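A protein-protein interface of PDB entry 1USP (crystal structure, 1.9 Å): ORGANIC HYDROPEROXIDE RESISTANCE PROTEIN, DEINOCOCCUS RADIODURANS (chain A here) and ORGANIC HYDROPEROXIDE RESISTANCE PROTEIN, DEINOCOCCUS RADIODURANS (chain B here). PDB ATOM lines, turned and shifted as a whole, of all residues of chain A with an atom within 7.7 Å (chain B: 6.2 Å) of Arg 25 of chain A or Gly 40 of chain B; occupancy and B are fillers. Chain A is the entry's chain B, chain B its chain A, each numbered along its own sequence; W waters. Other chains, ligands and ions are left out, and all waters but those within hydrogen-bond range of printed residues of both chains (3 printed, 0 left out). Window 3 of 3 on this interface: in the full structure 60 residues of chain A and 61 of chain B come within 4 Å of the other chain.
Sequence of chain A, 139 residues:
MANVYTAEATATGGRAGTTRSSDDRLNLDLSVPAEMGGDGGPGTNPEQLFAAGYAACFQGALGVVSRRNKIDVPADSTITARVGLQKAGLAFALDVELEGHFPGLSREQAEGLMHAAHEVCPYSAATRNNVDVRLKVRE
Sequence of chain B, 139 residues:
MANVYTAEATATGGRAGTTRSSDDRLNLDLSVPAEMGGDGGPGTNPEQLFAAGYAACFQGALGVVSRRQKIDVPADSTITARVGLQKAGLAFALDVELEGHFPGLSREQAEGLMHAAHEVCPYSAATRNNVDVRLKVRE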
ATOM      1  N   TYR A   5      37.699  -7.868 -15.858  1.00  0.00           N
ATOM      2  CA  TYR A   5      36.318  -7.397 -15.869  1.00  0.00           C
ATOM      3  C   TYR A   5      35.641  -8.065 -14.683  1.00  0.00           C
ATOM      4  O   TYR A   5      35.945  -9.197 -14.379  1.00  0.00           O
ATOM      5  CB  TYR A   5      35.624  -7.767 -17.182  1.00  0.00           C
ATOM      6  CG  TYR A   5      34.107  -7.668 -17.139  1.00  0.00           C
ATOM      7  CD1 TYR A   5      33.475  -6.425 -17.110  1.00  0.00           C
ATOM      8  CD2 TYR A   5      33.313  -8.810 -17.117  1.00  0.00           C
ATOM      9  CE1 TYR A   5      32.084  -6.324 -17.074  1.00  0.00           C
ATOM     10  CE2 TYR A   5      31.938  -8.727 -17.070  1.00  0.00           C
ATOM     11  CZ  TYR A   5      31.319  -7.476 -17.051  1.00  0.00           C
ATOM     12  OH  TYR A   5      29.945  -7.387 -17.004  1.00  0.00           O
ATOM     13  N   ARG A  20      19.243  -9.747 -10.989  1.00  0.00           N
ATOM     14  CA  ARG A  20      19.385  -8.490 -11.686  1.00  0.00           C
ATOM     15  C   ARG A  20      20.801  -7.996 -11.583  1.00  0.00           C
ATOM     16  O   ARG A  20      21.333  -7.841 -10.463  1.00  0.00           O
ATOM     17  CB  ARG A  20      18.449  -7.485 -11.030  1.00  0.00           C
ATOM     18  CG  ARG A  20      18.301  -6.180 -11.772  1.00  0.00           C
ATOM     19  CD  ARG A  20      17.309  -5.274 -11.088  1.00  0.00           C
ATOM     20  NE  ARG A  20      17.062  -4.060 -11.859  1.00  0.00           N
ATOM     21  CZ  ARG A  20      15.892  -3.431 -11.898  1.00  0.00           C
ATOM     22  NH1 ARG A  20      14.849  -3.898 -11.225  1.00  0.00           N
ATOM     23  NH2 ARG A  20      15.761  -2.330 -12.620  1.00  0.00           N
ATOM     24  N   SER A  21      21.429  -7.753 -12.729  1.00  0.00           N
ATOM     25  CA  SER A  21      22.792  -7.259 -12.729  1.00  0.00           C
ATOM     26  C   SER A  21      22.834  -5.791 -12.335  1.00  0.00           C
ATOM     27  O   SER A  21      21.849  -5.062 -12.456  1.00  0.00           O
ATOM     28  CB  SER A  21      23.474  -7.483 -14.079  1.00  0.00           C
ATOM     29  OG  SER A  21      22.778  -6.844 -15.133  1.00  0.00           O
ATOM     30  N   SER A  22      24.004  -5.354 -11.898  1.00  0.00           N
ATOM     31  CA  SER A  22      24.193  -3.989 -11.420  1.00  0.00           C
ATOM     32  C   SER A  22      24.075  -2.929 -12.530  1.00  0.00           C
ATOM     33  O   SER A  22      23.908  -1.762 -12.224  1.00  0.00           O
ATOM     34  CB  SER A  22      25.548  -3.861 -10.749  1.00  0.00           C
ATOM     35  OG  SER A  22      26.572  -4.107 -11.673  1.00  0.00           O
ATOM     36  N   ASP A  23      24.199  -3.341 -13.789  1.00  0.00           N
ATOM     37  CA  ASP A  23      24.008  -2.453 -14.956  1.00  0.00           C
ATOM     38  C   ASP A  23      22.665  -2.622 -15.669  1.00  0.00           C
ATOM     39  O   ASP A  23      22.406  -1.991 -16.708  1.00  0.00           O
ATOM     40  CB  ASP A  23      25.153  -2.636 -15.955  1.00  0.00           C
ATOM     41  CG  ASP A  23      25.280  -4.072 -16.442  1.00  0.00           C
ATOM     42  OD1 ASP A  23      24.351  -4.898 -16.203  1.00  0.00           O
ATOM     43  OD2 ASP A  23      26.306  -4.465 -17.047  1.00  0.00           O
ATOM     44  N   ASP A  24      21.788  -3.433 -15.086  1.00  0.00           N
ATOM     45  CA  ASP A  24      20.507  -3.811 -15.665  1.00  0.00           C
ATOM     46  C   ASP A  24      20.536  -4.573 -16.995  1.00  0.00           C
ATOM     47  O   ASP A  24      19.470  -4.801 -17.551  1.00  0.00           O
ATOM     48  CB  ASP A  24      19.594  -2.587 -15.808  1.00  0.00           C
ATOM     49  CG  ASP A  24      18.777  -2.330 -14.571  1.00  0.00           C
ATOM     50  OD1 ASP A  24      19.165  -2.811 -13.456  1.00  0.00           O
ATOM     51  OD2 ASP A  24      17.752  -1.615 -14.631  1.00  0.00           O
ATOM     52  N   ARG A  25      21.710  -4.978 -17.486  1.00  0.00           N
ATOM     53  CA  ARG A  25      21.785  -5.815 -18.696  1.00  0.00           C
ATOM     54  C   ARG A  25      21.016  -7.128 -18.554  1.00  0.00           C
ATOM     55  O   ARG A  25      20.473  -7.670 -19.544  1.00  0.00           O
ATOM     56  CB  ARG A  25      23.223  -6.085 -19.095  1.00  0.00           C
ATOM     57  CG  ARG A  25      23.895  -4.873 -19.729  1.00  0.00           C
ATOM     58  CD  ARG A  25      25.343  -5.113 -20.125  1.00  0.00           C
ATOM     59  NE  ARG A  25      25.897  -4.051 -20.981  1.00  0.00           N
ATOM     60  CZ  ARG A  25      26.548  -2.961 -20.565  1.00  0.00           C
ATOM     61  NH1 ARG A  25      26.762  -2.712 -19.278  1.00  0.00           N
ATOM     62  NH2 ARG A  25      27.012  -2.091 -21.450  1.00  0.00           N
ATOM     63  N   LEU A  26      21.015  -7.646 -17.331  1.00  0.00           N
ATOM     64  CA  LEU A  26      20.141  -8.734 -16.934  1.00  0.00           C
ATOM     65  C   LEU A  26      19.207  -8.198 -15.876  1.00  0.00           C
ATOM     66  O   LEU A  26      19.652  -7.632 -14.866  1.00  0.00           O
ATOM     67  CB  LEU A  26      20.932  -9.886 -16.335  1.00  0.00           C
ATOM     68  CG  LEU A  26      21.894 -10.635 -17.240  1.00  0.00           C
ATOM     69  CD1 LEU A  26      22.453 -11.811 -16.437  1.00  0.00           C
ATOM     70  CD2 LEU A  26      21.219 -11.123 -18.511  1.00  0.00           C
ATOM     71  N   ASN A  27      17.917  -8.404 -16.104  1.00  0.00           N
ATOM     72  CA  ASN A  27      16.884  -7.993 -15.176  1.00  0.00           C
ATOM     73  C   ASN A  27      15.771  -9.020 -15.316  1.00  0.00           C
ATOM     74  O   ASN A  27      14.894  -8.899 -16.182  1.00  0.00           O
ATOM     75  CB  ASN A  27      16.436  -6.558 -15.518  1.00  0.00           C
ATOM     76  CG  ASN A  27      15.299  -6.066 -14.647  1.00  0.00           C
ATOM     77  OD1 ASN A  27      14.926  -6.705 -13.663  1.00  0.00           O
ATOM     78  ND2 ASN A  27      14.747  -4.894 -15.006  1.00  0.00           N
ATOM     79  N   LEU A  28      15.843 -10.063 -14.494  1.00  0.00           N
ATOM     80  CA  LEU A  28      15.112 -11.296 -14.741  1.00  0.00           C
ATOM     81  C   LEU A  28      14.280 -11.713 -13.535  1.00  0.00           C
ATOM     82  O   LEU A  28      14.657 -11.446 -12.393  1.00  0.00           O
ATOM     83  CB  LEU A  28      16.087 -12.428 -15.098  1.00  0.00           C
ATOM     84  CG  LEU A  28      16.893 -12.281 -16.395  1.00  0.00           C
ATOM     85  CD1 LEU A  28      18.010 -13.315 -16.457  1.00  0.00           C
ATOM     86  CD2 LEU A  28      16.001 -12.403 -17.618  1.00  0.00           C
ATOM     87  N   LEU B  28      18.469 -13.646 -24.783  1.00  0.00           N
ATOM     88  CA  LEU B  28      19.437 -12.628 -24.425  1.00  0.00           C
ATOM     89  C   LEU B  28      20.424 -12.359 -25.523  1.00  0.00           C
ATOM     90  O   LEU B  28      20.916 -13.263 -26.184  1.00  0.00           O
ATOM     91  CB  LEU B  28      20.189 -13.060 -23.171  1.00  0.00           C
ATOM     92  CG  LEU B  28      19.276 -13.329 -21.980  1.00  0.00           C
ATOM     93  CD1 LEU B  28      20.014 -14.116 -20.892  1.00  0.00           C
ATOM     94  CD2 LEU B  28      18.754 -11.992 -21.455  1.00  0.00           C
ATOM     95  N   SER B  31      27.050  -9.121 -25.480  1.00  0.00           N
ATOM     96  CA  SER B  31      28.001  -8.095 -25.873  1.00  0.00           C
ATOM     97  C   SER B  31      29.282  -8.294 -25.093  1.00  0.00           C
ATOM     98  O   SER B  31      29.254  -8.672 -23.905  1.00  0.00           O
ATOM     99  CB  SER B  31      27.457  -6.676 -25.591  1.00  0.00           C
ATOM    100  OG  SER B  31      26.242  -6.417 -26.267  1.00  0.00           O
ATOM    101  N   VAL B  32      30.412  -8.034 -25.748  1.00  0.00           N
ATOM    102  CA  VAL B  32      31.694  -8.058 -25.065  1.00  0.00           C
ATOM    103  C   VAL B  32      31.899  -6.712 -24.383  1.00  0.00           C
ATOM    104  O   VAL B  32      31.760  -5.660 -25.029  1.00  0.00           O
ATOM    105  CB  VAL B  32      32.866  -8.369 -26.018  1.00  0.00           C
ATOM    106  CG1 VAL B  32      34.181  -8.380 -25.245  1.00  0.00           C
ATOM    107  CG2 VAL B  32      32.649  -9.703 -26.717  1.00  0.00           C
ATOM    108  N   PRO B  33      32.172  -6.721 -23.077  1.00  0.00           N
ATOM    109  CA  PRO B  33      32.375  -5.470 -22.338  1.00  0.00           C
ATOM    110  C   PRO B  33      33.548  -4.621 -22.835  1.00  0.00           C
ATOM    111  O   PRO B  33      34.576  -5.138 -23.285  1.00  0.00           O
ATOM    112  CB  PRO B  33      32.595  -5.932 -20.899  1.00  0.00           C
ATOM    113  CG  PRO B  33      31.967  -7.302 -20.840  1.00  0.00           C
ATOM    114  CD  PRO B  33      32.219  -7.897 -22.189  1.00  0.00           C
ATOM    115  N   ALA B  34      33.355  -3.308 -22.768  1.00  0.00           N
ATOM    116  CA  ALA B  34      34.370  -2.331 -23.154  1.00  0.00           C
ATOM    117  C   ALA B  34      35.689  -2.561 -22.422  1.00  0.00           C
ATOM    118  O   ALA B  34      36.754  -2.299 -22.968  1.00  0.00           O
ATOM    119  CB  ALA B  34      33.857  -0.932 -22.890  1.00  0.00           C
ATOM    120  N   GLY B  38      35.643  -4.924 -26.135  1.00  0.00           N
ATOM    121  CA  GLY B  38      34.402  -5.047 -26.879  1.00  0.00           C
ATOM    122  C   GLY B  38      33.734  -3.699 -27.013  1.00  0.00           C
ATOM    123  O   GLY B  38      34.238  -2.710 -26.506  1.00  0.00           O
ATOM    124  N   ASP B  39      32.581  -3.666 -27.670  1.00  0.00           N
ATOM    125  CA  ASP B  39      31.868  -2.407 -27.917  1.00  0.00           C
ATOM    126  C   ASP B  39      31.030  -1.893 -26.720  1.00  0.00           C
ATOM    127  O   ASP B  39      30.508  -0.786 -26.769  1.00  0.00           O
ATOM    128  CB  ASP B  39      31.015  -2.493 -29.199  1.00  0.00           C
ATOM    129  CG  ASP B  39      29.888  -3.535 -29.129  1.00  0.00           C
ATOM    130  OD1 ASP B  39      29.611  -4.128 -28.055  1.00  0.00           O
ATOM    131  OD2 ASP B  39      29.213  -3.824 -30.142  1.00  0.00           O
ATOM    132  N   GLY B  40      30.919  -2.684 -25.652  1.00  0.00           N
ATOM    133  CA  GLY B  40      30.166  -2.264 -24.476  1.00  0.00           C
ATOM    134  C   GLY B  40      28.677  -2.112 -24.741  1.00  0.00           C
ATOM    135  O   GLY B  40      28.021  -1.264 -24.145  1.00  0.00           O
ATOM    136  N   GLY B  41      28.151  -2.938 -25.642  1.00  0.00           N
ATOM    137  CA  GLY B  41      26.747  -2.928 -25.990  1.00  0.00           C
ATOM    138  C   GLY B  41      25.863  -3.459 -24.872  1.00  0.00           C
ATOM    139  O   GLY B  41      26.369  -3.898 -23.837  1.00  0.00           O
ATOM    140  N   PRO B  42      24.555  -3.435 -25.089  1.00  0.00           N
ATOM    141  CA  PRO B  42      23.558  -3.769 -24.053  1.00  0.00           C
ATOM    142  C   PRO B  42      23.387  -5.263 -23.758  1.00  0.00           C
ATOM    143  O   PRO B  42      22.653  -5.611 -22.828  1.00  0.00           O
ATOM    144  CB  PRO B  42      22.250  -3.222 -24.649  1.00  0.00           C
ATOM    145  CG  PRO B  42      22.454  -3.362 -26.174  1.00  0.00           C
ATOM    146  CD  PRO B  42      23.921  -3.085 -26.382  1.00  0.00           C
ATOM    147  N   GLY B  43      23.988  -6.131 -24.570  1.00  0.00           N
ATOM    148  CA  GLY B  43      23.974  -7.561 -24.313  1.00  0.00           C
ATOM    149  C   GLY B  43      24.768  -7.926 -23.068  1.00  0.00           C
ATOM    150  O   GLY B  43      25.634  -7.157 -22.623  1.00  0.00           O
ATOM    151  N   THR B  44      24.442  -9.084 -22.498  1.00  0.00           N
ATOM    152  CA  THR B  44      25.088  -9.615 -21.300  1.00  0.00           C
ATOM    153  C   THR B  44      26.335 -10.383 -21.712  1.00  0.00           C
ATOM    154  O   THR B  44      26.779 -10.308 -22.867  1.00  0.00           O
ATOM    155  CB  THR B  44      24.055 -10.472 -20.470  1.00  0.00           C
ATOM    156  OG1 THR B  44      24.622 -10.893 -19.229  1.00  0.00           O
ATOM    157  CG2 THR B  44      23.704 -11.770 -21.165  1.00  0.00           C
ATOM    158  N   ASN B  45      26.952 -11.071 -20.757  1.00  0.00           N
ATOM    159  CA  ASN B  45      28.169 -11.820 -21.009  1.00  0.00           C
ATOM    160  C   ASN B  45      28.224 -13.014 -20.037  1.00  0.00           C
ATOM    161  O   ASN B  45      27.438 -13.065 -19.081  1.00  0.00           O
ATOM    162  CB  ASN B  45      29.366 -10.877 -20.843  1.00  0.00           C
ATOM    163  CG  ASN B  45      29.422 -10.263 -19.462  1.00  0.00           C
ATOM    164  OD1 ASN B  45      29.707 -10.955 -18.492  1.00  0.00           O
ATOM    165  ND2 ASN B  45      29.149  -8.966 -19.361  1.00  0.00           N
ATOM    166  N   GLN B  48      28.678 -12.256 -16.202  1.00  0.00           N
ATOM    167  CA  GLN B  48      27.447 -11.693 -15.703  1.00  0.00           C
ATOM    168  C   GLN B  48      26.341 -12.725 -15.557  1.00  0.00           C
ATOM    169  O   GLN B  48      25.570 -12.708 -14.590  1.00  0.00           O
ATOM    170  CB  GLN B  48      27.013 -10.560 -16.618  1.00  0.00           C
ATOM    171  CG  GLN B  48      26.034  -9.644 -15.993  1.00  0.00           C
ATOM    172  CD  GLN B  48      25.744  -8.439 -16.861  1.00  0.00           C
ATOM    173  OE1 GLN B  48      25.082  -8.565 -17.910  1.00  0.00           O
ATOM    174  NE2 GLN B  48      26.233  -7.263 -16.433  1.00  0.00           N
HETATM  175  O   HOH W   1      27.390  -6.281 -13.755  1.00  0.00           O
HETATM  176  O   HOH W   2      21.104  -7.479 -22.069  1.00  0.00           O
HETATM  177  O   HOH W   3      28.661  -4.903 -22.614  1.00  0.00           O
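Of the printed residues of chain B, Tyr 5 of chain A touches Pro 33 (3.8 Å), Asn 45 (2.9 Å) and Gln 48 (3.8 Å).
Of the printed residues of chain B, Ser 21 of chain A touches Gln 48 (3.6 Å).
Asn 27 of chain A touches none of the printed residues of chain B.
Gly 38 of chain B touches none of the printed residues of chain A.
Of chain A, only Arg 25 (3.0 Å) comes within 4 Å of Gly 40 of chain B.
Gly 41 of chain B touches one residue of chain A.
Of the printed residues of chain A, Thr 44 of chain B touches Leu 26.
The nearest residue of chain B that does not touch Arg 25 of chain A is Thr 44 of chain B (4.6 Å).
Water W2 lies within hydrogen-bond range of the backbone carbonyl oxygen (O) of Pro 42 of chain B (2.5 Å) and the backbone carbonyl oxygen (O) of Arg 25 of chain A (2.6 Å).
Water W3 lies within hydrogen-bond range of O of Gly 41 of chain B (2.8 Å) and NE of Arg 25 of chain A (3.3 Å).
Water W1 bridges the side-chain amide nitrogen (NE2) of Gln 48 of chain B (3.1 Å) and the side-chain hydroxyl (OG) of Ser 22 of chain A (3.1 Å).
Hydrophobic or aromatic side chains of chain B that line the printed part of chain A: Leu 28 and Pro 33.
Of the 10 printed residues of chain A, 5 touch a printed residue of chain B.
Printed residues of chain A that touch a printed residue of chain B: Tyr 5, Ser 21, Asp 23, Arg 25 and Leu 26.
Among the printed residues, no Asp or Glu carboxylate lies within 4 Å of a Lys or Arg side-chain nitrogen of the other chain.
OE1 of Gln 48 of chain B lies within hydrogen-bond range of OG1 of Thr 44 of chain B (2.7 Å).
N of Arg 25 of chain A sits at hydrogen-bond distance from OG of Ser 21 of chain A, 3.2 Å away.
O of Val 32 of chain B is in hydrogen-bond range of N of Gly 40 of chain B, at 3.2 Å.
OD2 of Asp 23 of chain A lies within salt-bridge range of NH1 of Arg 25 of chain A, 2.9 Å away.
The backbone NH (N) of Gly 43 of chain B lies within hydrogen-bond range of the side-chain hydroxyl (OG) of Ser 31 of chain B (2.8 Å).
The side-chain amide oxygen (OD1) of Asn 45 of chain B sits at hydrogen-bond distance from the backbone NH (N) of Gln 48 of chain B, 2.8 Å away.
Among the printed residues, pairs that only touch across the chains: Arg 25 of chain A with Gly 43 of chain B, Arg 25 of chain A with Gln 48 of chain B, Leu 26 of chain A with Thr 44 of chain B, Arg 25 of chain A with Pro 42 of chain B, Ser 21 of chain A with Gln 48 of chain B, Leu 26 of chain A with Gln 48 of chain B, Tyr 5 of chain A with Gln 48 of chain B, Tyr 5 of chain A with Pro 33 of chain B and Leu 26 of chain A with Leu 28 of chain B.
The side-chain amide nitrogen (ND2) of Asn 45 of chain B is in hydrogen-bond range of the side-chain hydroxyl (OH) of Tyr 5 of chain A, at 2.9 Å.
The side-chain carboxylate (OD2) of Asp 23 of chain A lies within hydrogen-bond range of the side-chain amide nitrogen (NE2) of Gln 48 of chain B, at 2.9 Å.
O of Gly 41 of chain B sits at hydrogen-bond distance from NE of Arg 25 of chain A (2.9 Å).
The guanidinium group of Arg 25 of chain A is in hydrogen-bond range of the backbone carbonyl oxygen of Gly 40 of chain B.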
